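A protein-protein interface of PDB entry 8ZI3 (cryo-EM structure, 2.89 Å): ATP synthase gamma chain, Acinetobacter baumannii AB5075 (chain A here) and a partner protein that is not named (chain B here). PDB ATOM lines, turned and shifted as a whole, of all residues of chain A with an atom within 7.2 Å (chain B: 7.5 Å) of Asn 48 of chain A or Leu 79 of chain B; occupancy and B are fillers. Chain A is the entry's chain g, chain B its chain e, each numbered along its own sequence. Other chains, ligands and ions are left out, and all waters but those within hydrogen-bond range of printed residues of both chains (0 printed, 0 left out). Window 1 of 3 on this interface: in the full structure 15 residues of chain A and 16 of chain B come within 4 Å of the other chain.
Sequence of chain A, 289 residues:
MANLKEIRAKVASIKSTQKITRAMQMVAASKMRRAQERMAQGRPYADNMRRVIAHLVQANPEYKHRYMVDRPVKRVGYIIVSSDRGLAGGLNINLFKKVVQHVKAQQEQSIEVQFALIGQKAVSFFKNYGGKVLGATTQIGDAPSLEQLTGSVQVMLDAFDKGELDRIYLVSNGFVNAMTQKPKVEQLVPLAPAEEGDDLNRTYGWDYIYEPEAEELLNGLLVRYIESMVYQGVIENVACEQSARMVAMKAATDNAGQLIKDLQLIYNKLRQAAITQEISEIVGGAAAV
OD1 of Asp 81 of chain B lies within salt-bridge range of NH1 of Arg 224 of chain A. The side-chain hydroxyl (OH) of Tyr 45 of chain A is in hydrogen-bond range of the backbone carbonyl oxygen (O) of Ser 10 of chain B, 3.2 Å away.
The backbone carbonyl oxygen of Gly 66 of chain B sits at hydrogen-bond distance from the backbone NH of Asp 81 of chain B, 2.6 Å away. O of Leu 45 of chain B sits at hydrogen-bond distance from N of Gly 67 of chain B, 3.2 Å away. The backbone NH of Val 9 of chain B lies within hydrogen-bond range of the backbone carbonyl oxygen of Val 78 of chain B (3.1 Å). The backbone NH (N) of Val 68 of chain B is in hydrogen-bond range of the backbone carbonyl oxygen (O) of Leu 79 of chain B (2.6 Å).
Among the printed residues, merely in contact across the chains: Asn 48 of chain A with Leu 79 of chain B, Tyr 45 of chain A with Val 9 of chain B, Tyr 45 of chain A with Leu 79 of chain B, Arg 224 of chain A with Leu 79 of chain B, Arg 224 of chain A with Gly 67 of chain B and Arg 224 of chain A with Val 68 of chain B.
Of the printed residues of chain B, Tyr 45 of chain A touches Val 9, Ser 10 and Leu 79. Asn 48 of chain A touches just one residue of chain B: Leu 79. Arg 51 of chain A touches none of the printed residues of chain B. Ala 54 of chain A touches none of the printed residues of chain B. Of the printed residues of chain B, Arg 224 of chain A touches Gly 67, Val 68, Leu 79 and Asp 81. Of the printed residues of chain A, Val 9 of chain B touches Tyr 45 (3.5 Å). Of the printed residues of chain A, Gly 67 of chain B touches Arg 224. Of chain A, only Tyr 45, Asn 48 and Arg 224 come within 4 Å of Leu 79 of chain B.
Of the 19 printed residues of chain B, 6 touch a printed residue of chain A. Printed residues of chain B that touch a printed residue of chain A: Val 9, Ser 10, Gly 67, Val 68, Leu 79 and Asp 81. Of the 14 printed residues of chain A, 3 touch a printed residue of chain B. Printed residues of chain A that touch a printed residue of chain B: Tyr 45, Asn 48 and Arg 224. Along chain A the printed residues that touch a printed residue of chain B span positions 45 to 224. Among the printed residues, Asp or Glu carboxylates within 4 Å of a Lys or Arg side-chain nitrogen of the other chain: Arg 224 of chain A with Asp 81 of chain B (3.3 Å).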
ATOM      1  N   ARG A  43     -18.115  -4.359 -27.013  1.00  0.00           N
ATOM      2  CA  ARG A  43     -17.638  -4.411 -28.396  1.00  0.00           C
ATOM      3  C   ARG A  43     -16.133  -4.195 -28.551  1.00  0.00           C
ATOM      4  O   ARG A  43     -15.508  -4.933 -29.338  1.00  0.00           O
ATOM      5  CB  ARG A  43     -18.427  -3.402 -29.239  1.00  0.00           C
ATOM      6  CG  ARG A  43     -19.759  -3.932 -29.744  1.00  0.00           C
ATOM      7  CD  ARG A  43     -20.695  -2.802 -30.144  1.00  0.00           C
ATOM      8  NE  ARG A  43     -20.567  -2.452 -31.553  1.00  0.00           N
ATOM      9  CZ  ARG A  43     -21.184  -3.088 -32.541  1.00  0.00           C
ATOM     10  NH1 ARG A  43     -21.980  -4.119 -32.308  1.00  0.00           N
ATOM     11  NH2 ARG A  43     -20.998  -2.679 -33.792  1.00  0.00           N
ATOM     12  N   PRO A  44     -15.495  -3.218 -27.888  1.00  0.00           N
ATOM     13  CA  PRO A  44     -14.053  -3.017 -28.117  1.00  0.00           C
ATOM     14  C   PRO A  44     -13.198  -4.233 -27.801  1.00  0.00           C
ATOM     15  O   PRO A  44     -12.160  -4.420 -28.444  1.00  0.00           O
ATOM     16  CB  PRO A  44     -13.710  -1.830 -27.203  1.00  0.00           C
ATOM     17  CG  PRO A  44     -14.838  -1.734 -26.238  1.00  0.00           C
ATOM     18  CD  PRO A  44     -16.040  -2.179 -26.999  1.00  0.00           C
ATOM     19  N   TYR A  45     -13.594  -5.064 -26.835  1.00  0.00           N
ATOM     20  CA  TYR A  45     -12.855  -6.299 -26.584  1.00  0.00           C
ATOM     21  C   TYR A  45     -12.907  -7.216 -27.800  1.00  0.00           C
ATOM     22  O   TYR A  45     -11.897  -7.819 -28.186  1.00  0.00           O
ATOM     23  CB  TYR A  45     -13.416  -7.007 -25.350  1.00  0.00           C
ATOM     24  CG  TYR A  45     -12.628  -8.227 -24.920  1.00  0.00           C
ATOM     25  CD1 TYR A  45     -11.238  -8.219 -24.919  1.00  0.00           C
ATOM     26  CD2 TYR A  45     -13.274  -9.388 -24.512  1.00  0.00           C
ATOM     27  CE1 TYR A  45     -10.517  -9.330 -24.521  1.00  0.00           C
ATOM     28  CE2 TYR A  45     -12.561 -10.503 -24.115  1.00  0.00           C
ATOM     29  CZ  TYR A  45     -11.183 -10.469 -24.122  1.00  0.00           C
ATOM     30  OH  TYR A  45     -10.470 -11.579 -23.727  1.00  0.00           O
ATOM     31  N   ALA A  46     -14.084  -7.332 -28.420  1.00  0.00           N
ATOM     32  CA  ALA A  46     -14.211  -8.141 -29.627  1.00  0.00           C
ATOM     33  C   ALA A  46     -13.378  -7.567 -30.766  1.00  0.00           C
ATOM     34  O   ALA A  46     -12.744  -8.315 -31.520  1.00  0.00           O
ATOM     35  CB  ALA A  46     -15.681  -8.247 -30.035  1.00  0.00           C
ATOM     36  N   ASP A  47     -13.373  -6.239 -30.912  1.00  0.00           N
ATOM     37  CA  ASP A  47     -12.549  -5.621 -31.948  1.00  0.00           C
ATOM     38  C   ASP A  47     -11.067  -5.887 -31.705  1.00  0.00           C
ATOM     39  O   ASP A  47     -10.316  -6.191 -32.642  1.00  0.00           O
ATOM     40  CB  ASP A  47     -12.830  -4.120 -32.010  1.00  0.00           C
ATOM     41  CG  ASP A  47     -14.314  -3.806 -32.032  1.00  0.00           C
ATOM     42  OD1 ASP A  47     -15.073  -4.557 -32.680  1.00  0.00           O
ATOM     43  OD2 ASP A  47     -14.723  -2.812 -31.395  1.00  0.00           O
ATOM     44  N   ASN A  48     -10.633  -5.796 -30.446  1.00  0.00           N
ATOM     45  CA  ASN A  48      -9.243  -6.083 -30.111  1.00  0.00           C
ATOM     46  C   ASN A  48      -8.895  -7.532 -30.416  1.00  0.00           C
ATOM     47  O   ASN A  48      -7.804  -7.827 -30.917  1.00  0.00           O
ATOM     48  CB  ASN A  48      -8.988  -5.778 -28.634  1.00  0.00           C
ATOM     49  CG  ASN A  48      -7.594  -6.176 -28.187  1.00  0.00           C
ATOM     50  OD1 ASN A  48      -7.374  -7.291 -27.710  1.00  0.00           O
ATOM     51  ND2 ASN A  48      -6.649  -5.254 -28.315  1.00  0.00           N
ATOM     52  N   MET A  49      -9.804  -8.456 -30.110  1.00  0.00           N
ATOM     53  CA  MET A  49      -9.495  -9.861 -30.332  1.00  0.00           C
ATOM     54  C   MET A  49      -9.501 -10.201 -31.819  1.00  0.00           C
ATOM     55  O   MET A  49      -8.724 -11.054 -32.263  1.00  0.00           O
ATOM     56  CB  MET A  49     -10.469 -10.735 -29.551  1.00  0.00           C
ATOM     57  CG  MET A  49     -10.231 -12.211 -29.720  1.00  0.00           C
ATOM     58  SD  MET A  49     -10.232 -12.959 -28.085  1.00  0.00           S
ATOM     59  CE  MET A  49     -10.041 -14.685 -28.490  1.00  0.00           C
ATOM     60  N   ARG A  50     -10.355  -9.541 -32.603  1.00  0.00           N
ATOM     61  CA  ARG A  50     -10.268  -9.664 -34.054  1.00  0.00           C
ATOM     62  C   ARG A  50      -8.927  -9.151 -34.565  1.00  0.00           C
ATOM     63  O   ARG A  50      -8.292  -9.776 -35.428  1.00  0.00           O
ATOM     64  CB  ARG A  50     -11.412  -8.895 -34.709  1.00  0.00           C
ATOM     65  CG  ARG A  50     -11.500  -9.087 -36.206  1.00  0.00           C
ATOM     66  CD  ARG A  50     -11.841  -7.788 -36.918  1.00  0.00           C
ATOM     67  NE  ARG A  50     -10.733  -6.839 -36.891  1.00  0.00           N
ATOM     68  CZ  ARG A  50     -10.667  -5.785 -36.090  1.00  0.00           C
ATOM     69  NH1 ARG A  50     -11.640  -5.500 -35.240  1.00  0.00           N
ATOM     70  NH2 ARG A  50      -9.601  -4.992 -36.148  1.00  0.00           N
ATOM     71  N   ARG A  51      -8.477  -8.011 -34.038  1.00  0.00           N
ATOM     72  CA  ARG A  51      -7.170  -7.492 -34.421  1.00  0.00           C
ATOM     73  C   ARG A  51      -6.070  -8.489 -34.087  1.00  0.00           C
ATOM     74  O   ARG A  51      -5.160  -8.712 -34.893  1.00  0.00           O
ATOM     75  CB  ARG A  51      -6.910  -6.154 -33.732  1.00  0.00           C
ATOM     76  CG  ARG A  51      -5.708  -5.396 -34.276  1.00  0.00           C
ATOM     77  CD  ARG A  51      -4.957  -4.688 -33.157  1.00  0.00           C
ATOM     78  NE  ARG A  51      -4.671  -5.576 -32.036  1.00  0.00           N
ATOM     79  CZ  ARG A  51      -3.680  -6.457 -32.008  1.00  0.00           C
ATOM     80  NH1 ARG A  51      -2.854  -6.600 -33.032  1.00  0.00           N
ATOM     81  NH2 ARG A  51      -3.511  -7.211 -30.926  1.00  0.00           N
ATOM     82  N   VAL A  52      -6.146  -9.115 -32.910  1.00  0.00           N
ATOM     83  CA  VAL A  52      -5.080 -10.023 -32.496  1.00  0.00           C
ATOM     84  C   VAL A  52      -5.114 -11.322 -33.300  1.00  0.00           C
ATOM     85  O   VAL A  52      -4.060 -11.899 -33.595  1.00  0.00           O
ATOM     86  CB  VAL A  52      -5.135 -10.280 -30.975  1.00  0.00           C
ATOM     87  CG1 VAL A  52      -6.170 -11.331 -30.613  1.00  0.00           C
ATOM     88  CG2 VAL A  52      -3.762 -10.682 -30.455  1.00  0.00           C
ATOM     89  N   ILE A  53      -6.302 -11.806 -33.683  1.00  0.00           N
ATOM     90  CA  ILE A  53      -6.342 -13.019 -34.496  1.00  0.00           C
ATOM     91  C   ILE A  53      -5.819 -12.734 -35.899  1.00  0.00           C
ATOM     92  O   ILE A  53      -5.102 -13.557 -36.481  1.00  0.00           O
ATOM     93  CB  ILE A  53      -7.751 -13.647 -34.518  1.00  0.00           C
ATOM     94  CG1 ILE A  53      -8.777 -12.717 -35.161  1.00  0.00           C
ATOM     95  CG2 ILE A  53      -8.174 -14.062 -33.114  1.00  0.00           C
ATOM     96  CD1 ILE A  53     -10.008 -13.423 -35.678  1.00  0.00           C
ATOM     97  N   ALA A  54      -6.143 -11.563 -36.460  1.00  0.00           N
ATOM     98  CA  ALA A  54      -5.530 -11.178 -37.730  1.00  0.00           C
ATOM     99  C   ALA A  54      -4.016 -11.071 -37.590  1.00  0.00           C
ATOM    100  O   ALA A  54      -3.263 -11.527 -38.464  1.00  0.00           O
ATOM    101  CB  ALA A  54      -6.123  -9.858 -38.222  1.00  0.00           C
ATOM    102  N   LEU A 221      -6.901 -19.405 -27.547  1.00  0.00           N
ATOM    103  CA  LEU A 221      -7.489 -18.176 -28.066  1.00  0.00           C
ATOM    104  C   LEU A 221      -8.571 -18.466 -29.096  1.00  0.00           C
ATOM    105  O   LEU A 221      -9.522 -17.691 -29.219  1.00  0.00           O
ATOM    106  CB  LEU A 221      -6.411 -17.260 -28.654  1.00  0.00           C
ATOM    107  CG  LEU A 221      -5.467 -17.755 -29.751  1.00  0.00           C
ATOM    108  CD1 LEU A 221      -6.034 -17.476 -31.138  1.00  0.00           C
ATOM    109  CD2 LEU A 221      -4.087 -17.131 -29.598  1.00  0.00           C
ATOM    110  N   ARG A 224     -11.597 -19.230 -27.056  1.00  0.00           N
ATOM    111  CA  ARG A 224     -12.057 -17.953 -26.513  1.00  0.00           C
ATOM    112  C   ARG A 224     -12.791 -17.137 -27.572  1.00  0.00           C
ATOM    113  O   ARG A 224     -13.806 -16.495 -27.278  1.00  0.00           O
ATOM    114  CB  ARG A 224     -10.889 -17.144 -25.947  1.00  0.00           C
ATOM    115  CG  ARG A 224     -10.160 -17.760 -24.759  1.00  0.00           C
ATOM    116  CD  ARG A 224      -8.699 -17.315 -24.730  1.00  0.00           C
ATOM    117  NE  ARG A 224      -7.849 -18.242 -23.993  1.00  0.00           N
ATOM    118  CZ  ARG A 224      -7.060 -17.891 -22.986  1.00  0.00           C
ATOM    119  NH1 ARG A 224      -6.969 -16.634 -22.586  1.00  0.00           N
ATOM    120  NH2 ARG A 224      -6.344 -18.826 -22.367  1.00  0.00           N
ATOM    121  N   ASP B   7      -2.883  -2.205 -21.271  1.00  0.00           N
ATOM    122  CA  ASP B   7      -4.304  -2.527 -21.230  1.00  0.00           C
ATOM    123  C   ASP B   7      -4.497  -4.005 -20.922  1.00  0.00           C
ATOM    124  O   ASP B   7      -3.815  -4.859 -21.498  1.00  0.00           O
ATOM    125  CB  ASP B   7      -4.983  -2.179 -22.558  1.00  0.00           C
ATOM    126  CG  ASP B   7      -4.495  -0.865 -23.136  1.00  0.00           C
ATOM    127  OD1 ASP B   7      -4.144   0.039 -22.349  1.00  0.00           O
ATOM    128  OD2 ASP B   7      -4.460  -0.740 -24.378  1.00  0.00           O
ATOM    129  N   VAL B   8      -5.425  -4.300 -20.015  1.00  0.00           N
ATOM    130  CA  VAL B   8      -5.832  -5.667 -19.706  1.00  0.00           C
ATOM    131  C   VAL B   8      -7.353  -5.725 -19.737  1.00  0.00           C
ATOM    132  O   VAL B   8      -8.022  -4.992 -18.998  1.00  0.00           O
ATOM    133  CB  VAL B   8      -5.291  -6.143 -18.346  1.00  0.00           C
ATOM    134  CG1 VAL B   8      -5.854  -5.303 -17.211  1.00  0.00           C
ATOM    135  CG2 VAL B   8      -5.608  -7.617 -18.134  1.00  0.00           C
ATOM    136  N   VAL B   9      -7.899  -6.582 -20.598  1.00  0.00           N
ATOM    137  CA  VAL B   9      -9.340  -6.775 -20.725  1.00  0.00           C
ATOM    138  C   VAL B   9      -9.627  -8.261 -20.573  1.00  0.00           C
ATOM    139  O   VAL B   9      -9.091  -9.079 -21.330  1.00  0.00           O
ATOM    140  CB  VAL B   9      -9.881  -6.257 -22.069  1.00  0.00           C
ATOM    141  CG1 VAL B   9     -11.401  -6.206 -22.043  1.00  0.00           C
ATOM    142  CG2 VAL B   9      -9.304  -4.886 -22.389  1.00  0.00           C
ATOM    143  N   SER B  10     -10.469  -8.611 -19.602  1.00  0.00           N
ATOM    144  CA  SER B  10     -10.814 -10.010 -19.367  1.00  0.00           C
ATOM    145  C   SER B  10     -12.104 -10.400 -20.085  1.00  0.00           C
ATOM    146  O   SER B  10     -12.098 -11.284 -20.947  1.00  0.00           O
ATOM    147  CB  SER B  10     -10.933 -10.274 -17.861  1.00  0.00           C
ATOM    148  OG  SER B  10     -11.489 -11.554 -17.613  1.00  0.00           O
ATOM    149  N   THR B  43       2.852 -14.473 -23.939  1.00  0.00           N
ATOM    150  CA  THR B  43       2.970 -15.452 -22.869  1.00  0.00           C
ATOM    151  C   THR B  43       1.586 -15.866 -22.394  1.00  0.00           C
ATOM    152  O   THR B  43       0.619 -15.108 -22.505  1.00  0.00           O
ATOM    153  CB  THR B  43       3.765 -14.899 -21.673  1.00  0.00           C
ATOM    154  OG1 THR B  43       4.843 -14.086 -22.146  1.00  0.00           O
ATOM    155  CG2 THR B  43       4.340 -16.035 -20.836  1.00  0.00           C
ATOM    156  N   LEU B  44       1.500 -17.084 -21.861  1.00  0.00           N
ATOM    157  CA  LEU B  44       0.307 -17.537 -21.154  1.00  0.00           C
ATOM    158  C   LEU B  44       0.368 -17.001 -19.728  1.00  0.00           C
ATOM    159  O   LEU B  44       1.202 -17.439 -18.929  1.00  0.00           O
ATOM    160  CB  LEU B  44       0.219 -19.061 -21.171  1.00  0.00           C
ATOM    161  CG  LEU B  44      -1.062 -19.674 -20.601  1.00  0.00           C
ATOM    162  CD1 LEU B  44      -2.234 -19.450 -21.543  1.00  0.00           C
ATOM    163  CD2 LEU B  44      -0.869 -21.157 -20.323  1.00  0.00           C
ATOM    164  N   LEU B  45      -0.511 -16.055 -19.410  1.00  0.00           N
ATOM    165  CA  LEU B  45      -0.435 -15.362 -18.131  1.00  0.00           C
ATOM    166  C   LEU B  45      -0.772 -16.297 -16.976  1.00  0.00           C
ATOM    167  O   LEU B  45      -1.706 -17.100 -17.053  1.00  0.00           O
ATOM    168  CB  LEU B  45      -1.380 -14.161 -18.123  1.00  0.00           C
ATOM    169  CG  LEU B  45      -1.359 -13.294 -16.863  1.00  0.00           C
ATOM    170  CD1 LEU B  45       0.056 -12.834 -16.548  1.00  0.00           C
ATOM    171  CD2 LEU B  45      -2.294 -12.104 -17.012  1.00  0.00           C
ATOM    172  N   GLY B  66      -5.364 -15.581 -14.812  1.00  0.00           N
ATOM    173  CA  GLY B  66      -4.657 -16.210 -15.907  1.00  0.00           C
ATOM    174  C   GLY B  66      -5.243 -15.861 -17.265  1.00  0.00           C
ATOM    175  O   GLY B  66      -6.365 -15.375 -17.392  1.00  0.00           O
ATOM    176  N   GLY B  67      -4.452 -16.129 -18.301  1.00  0.00           N
ATOM    177  CA  GLY B  67      -4.849 -15.822 -19.661  1.00  0.00           C
ATOM    178  C   GLY B  67      -3.669 -15.703 -20.605  1.00  0.00           C
ATOM    179  O   GLY B  67      -2.653 -16.379 -20.422  1.00  0.00           O
ATOM    180  N   VAL B  68      -3.790 -14.848 -21.616  1.00  0.00           N
ATOM    181  CA  VAL B  68      -2.745 -14.642 -22.612  1.00  0.00           C
ATOM    182  C   VAL B  68      -2.276 -13.197 -22.525  1.00  0.00           C
ATOM    183  O   VAL B  68      -3.094 -12.270 -22.567  1.00  0.00           O
ATOM    184  CB  VAL B  68      -3.240 -14.974 -24.032  1.00  0.00           C
ATOM    185  CG1 VAL B  68      -2.282 -14.418 -25.075  1.00  0.00           C
ATOM    186  CG2 VAL B  68      -3.402 -16.477 -24.197  1.00  0.00           C
ATOM    187  N   LEU B  69      -0.965 -13.009 -22.403  1.00  0.00           N
ATOM    188  CA  LEU B  69      -0.356 -11.689 -22.343  1.00  0.00           C
ATOM    189  C   LEU B  69       0.414 -11.424 -23.629  1.00  0.00           C
ATOM    190  O   LEU B  69       1.159 -12.285 -24.105  1.00  0.00           O
ATOM    191  CB  LEU B  69       0.581 -11.569 -21.135  1.00  0.00           C
ATOM    192  CG  LEU B  69       1.102 -10.179 -20.755  1.00  0.00           C
ATOM    193  CD1 LEU B  69       1.286 -10.080 -19.249  1.00  0.00           C
ATOM    194  CD2 LEU B  69       2.410  -9.853 -21.466  1.00  0.00           C
ATOM    195  N   GLU B  70       0.228 -10.232 -24.188  1.00  0.00           N
ATOM    196  CA  GLU B  70       0.938  -9.800 -25.383  1.00  0.00           C
ATOM    197  C   GLU B  70       1.752  -8.556 -25.055  1.00  0.00           C
ATOM    198  O   GLU B  70       1.208  -7.571 -24.547  1.00  0.00           O
ATOM    199  CB  GLU B  70      -0.037  -9.513 -26.530  1.00  0.00           C
ATOM    200  CG  GLU B  70       0.628  -9.100 -27.833  1.00  0.00           C
ATOM    201  CD  GLU B  70       0.659  -7.594 -28.020  1.00  0.00           C
ATOM    202  OE1 GLU B  70      -0.059  -6.888 -27.281  1.00  0.00           O
ATOM    203  OE2 GLU B  70       1.400  -7.117 -28.905  1.00  0.00           O
ATOM    204  N   VAL B  75       3.124  -1.366 -27.742  1.00  0.00           N
ATOM    205  CA  VAL B  75       1.825  -2.034 -27.719  1.00  0.00           C
ATOM    206  C   VAL B  75       1.901  -3.172 -26.710  1.00  0.00           C
ATOM    207  O   VAL B  75       2.578  -4.179 -26.954  1.00  0.00           O
ATOM    208  CB  VAL B  75       1.414  -2.558 -29.103  1.00  0.00           C
ATOM    209  CG1 VAL B  75       0.206  -3.477 -28.987  1.00  0.00           C
ATOM    210  CG2 VAL B  75       1.118  -1.402 -30.047  1.00  0.00           C
ATOM    211  N   VAL B  76       1.212  -3.018 -25.582  1.00  0.00           N
ATOM    212  CA  VAL B  76       1.128  -4.056 -24.561  1.00  0.00           C
ATOM    213  C   VAL B  76      -0.343  -4.301 -24.264  1.00  0.00           C
ATOM    214  O   VAL B  76      -1.037  -3.408 -23.763  1.00  0.00           O
ATOM    215  CB  VAL B  76       1.885  -3.671 -23.279  1.00  0.00           C
ATOM    216  CG1 VAL B  76       1.579  -4.662 -22.165  1.00  0.00           C
ATOM    217  CG2 VAL B  76       3.378  -3.612 -23.549  1.00  0.00           C
ATOM    218  N   THR B  77      -0.818  -5.508 -24.569  1.00  0.00           N
ATOM    219  CA  THR B  77      -2.212  -5.882 -24.366  1.00  0.00           C
ATOM    220  C   THR B  77      -2.268  -7.212 -23.631  1.00  0.00           C
ATOM    221  O   THR B  77      -1.524  -8.140 -23.963  1.00  0.00           O
ATOM    222  CB  THR B  77      -2.963  -5.985 -25.697  1.00  0.00           C
ATOM    223  OG1 THR B  77      -2.265  -6.877 -26.575  1.00  0.00           O
ATOM    224  CG2 THR B  77      -3.077  -4.618 -26.356  1.00  0.00           C
ATOM    225  N   VAL B  78      -3.149  -7.303 -22.639  1.00  0.00           N
ATOM    226  CA  VAL B  78      -3.320  -8.508 -21.838  1.00  0.00           C
ATOM    227  C   VAL B  78      -4.737  -9.024 -22.045  1.00  0.00           C
ATOM    228  O   VAL B  78      -5.705  -8.269 -21.903  1.00  0.00           O
ATOM    229  CB  VAL B  78      -3.048  -8.244 -20.345  1.00  0.00           C
ATOM    230  CG1 VAL B  78      -2.904  -9.557 -19.594  1.00  0.00           C
ATOM    231  CG2 VAL B  78      -1.805  -7.384 -20.174  1.00  0.00           C
ATOM    232  N   LEU B  79      -4.854 -10.306 -22.381  1.00  0.00           N
ATOM    233  CA  LEU B  79      -6.138 -10.968 -22.601  1.00  0.00           C
ATOM    234  C   LEU B  79      -6.230 -12.124 -21.608  1.00  0.00           C
ATOM    235  O   LEU B  79      -5.757 -13.230 -21.880  1.00  0.00           O
ATOM    236  CB  LEU B  79      -6.267 -11.448 -24.045  1.00  0.00           C
ATOM    237  CG  LEU B  79      -5.972 -10.405 -25.125  1.00  0.00           C
ATOM    238  CD1 LEU B  79      -6.079 -11.020 -26.512  1.00  0.00           C
ATOM    239  CD2 LEU B  79      -6.902  -9.209 -24.989  1.00  0.00           C
ATOM    240  N   ALA B  80      -6.841 -11.863 -20.458  1.00  0.00           N
ATOM    241  CA  ALA B  80      -6.928 -12.831 -19.380  1.00  0.00           C
ATOM    242  C   ALA B  80      -8.327 -13.447 -19.330  1.00  0.00           C
ATOM    243  O   ALA B  80      -9.188 -13.167 -20.169  1.00  0.00           O
ATOM    244  CB  ALA B  80      -6.552 -12.168 -18.054  1.00  0.00           C
ATOM    245  N   ASP B  81      -8.555 -14.298 -18.331  1.00  0.00           N
ATOM    246  CA  ASP B  81      -9.846 -14.929 -18.106  1.00  0.00           C
ATOM    247  C   ASP B  81     -10.311 -14.635 -16.688  1.00  0.00           C
ATOM    248  O   ASP B  81      -9.508 -14.594 -15.751  1.00  0.00           O
ATOM    249  CB  ASP B  81      -9.783 -16.449 -18.326  1.00  0.00           C
ATOM    250  CG  ASP B  81      -9.333 -16.819 -19.725  1.00  0.00           C
ATOM    251  OD1 ASP B  81      -9.509 -15.996 -20.647  1.00  0.00           O
ATOM    252  OD2 ASP B  81      -8.806 -17.937 -19.903  1.00  0.00           O
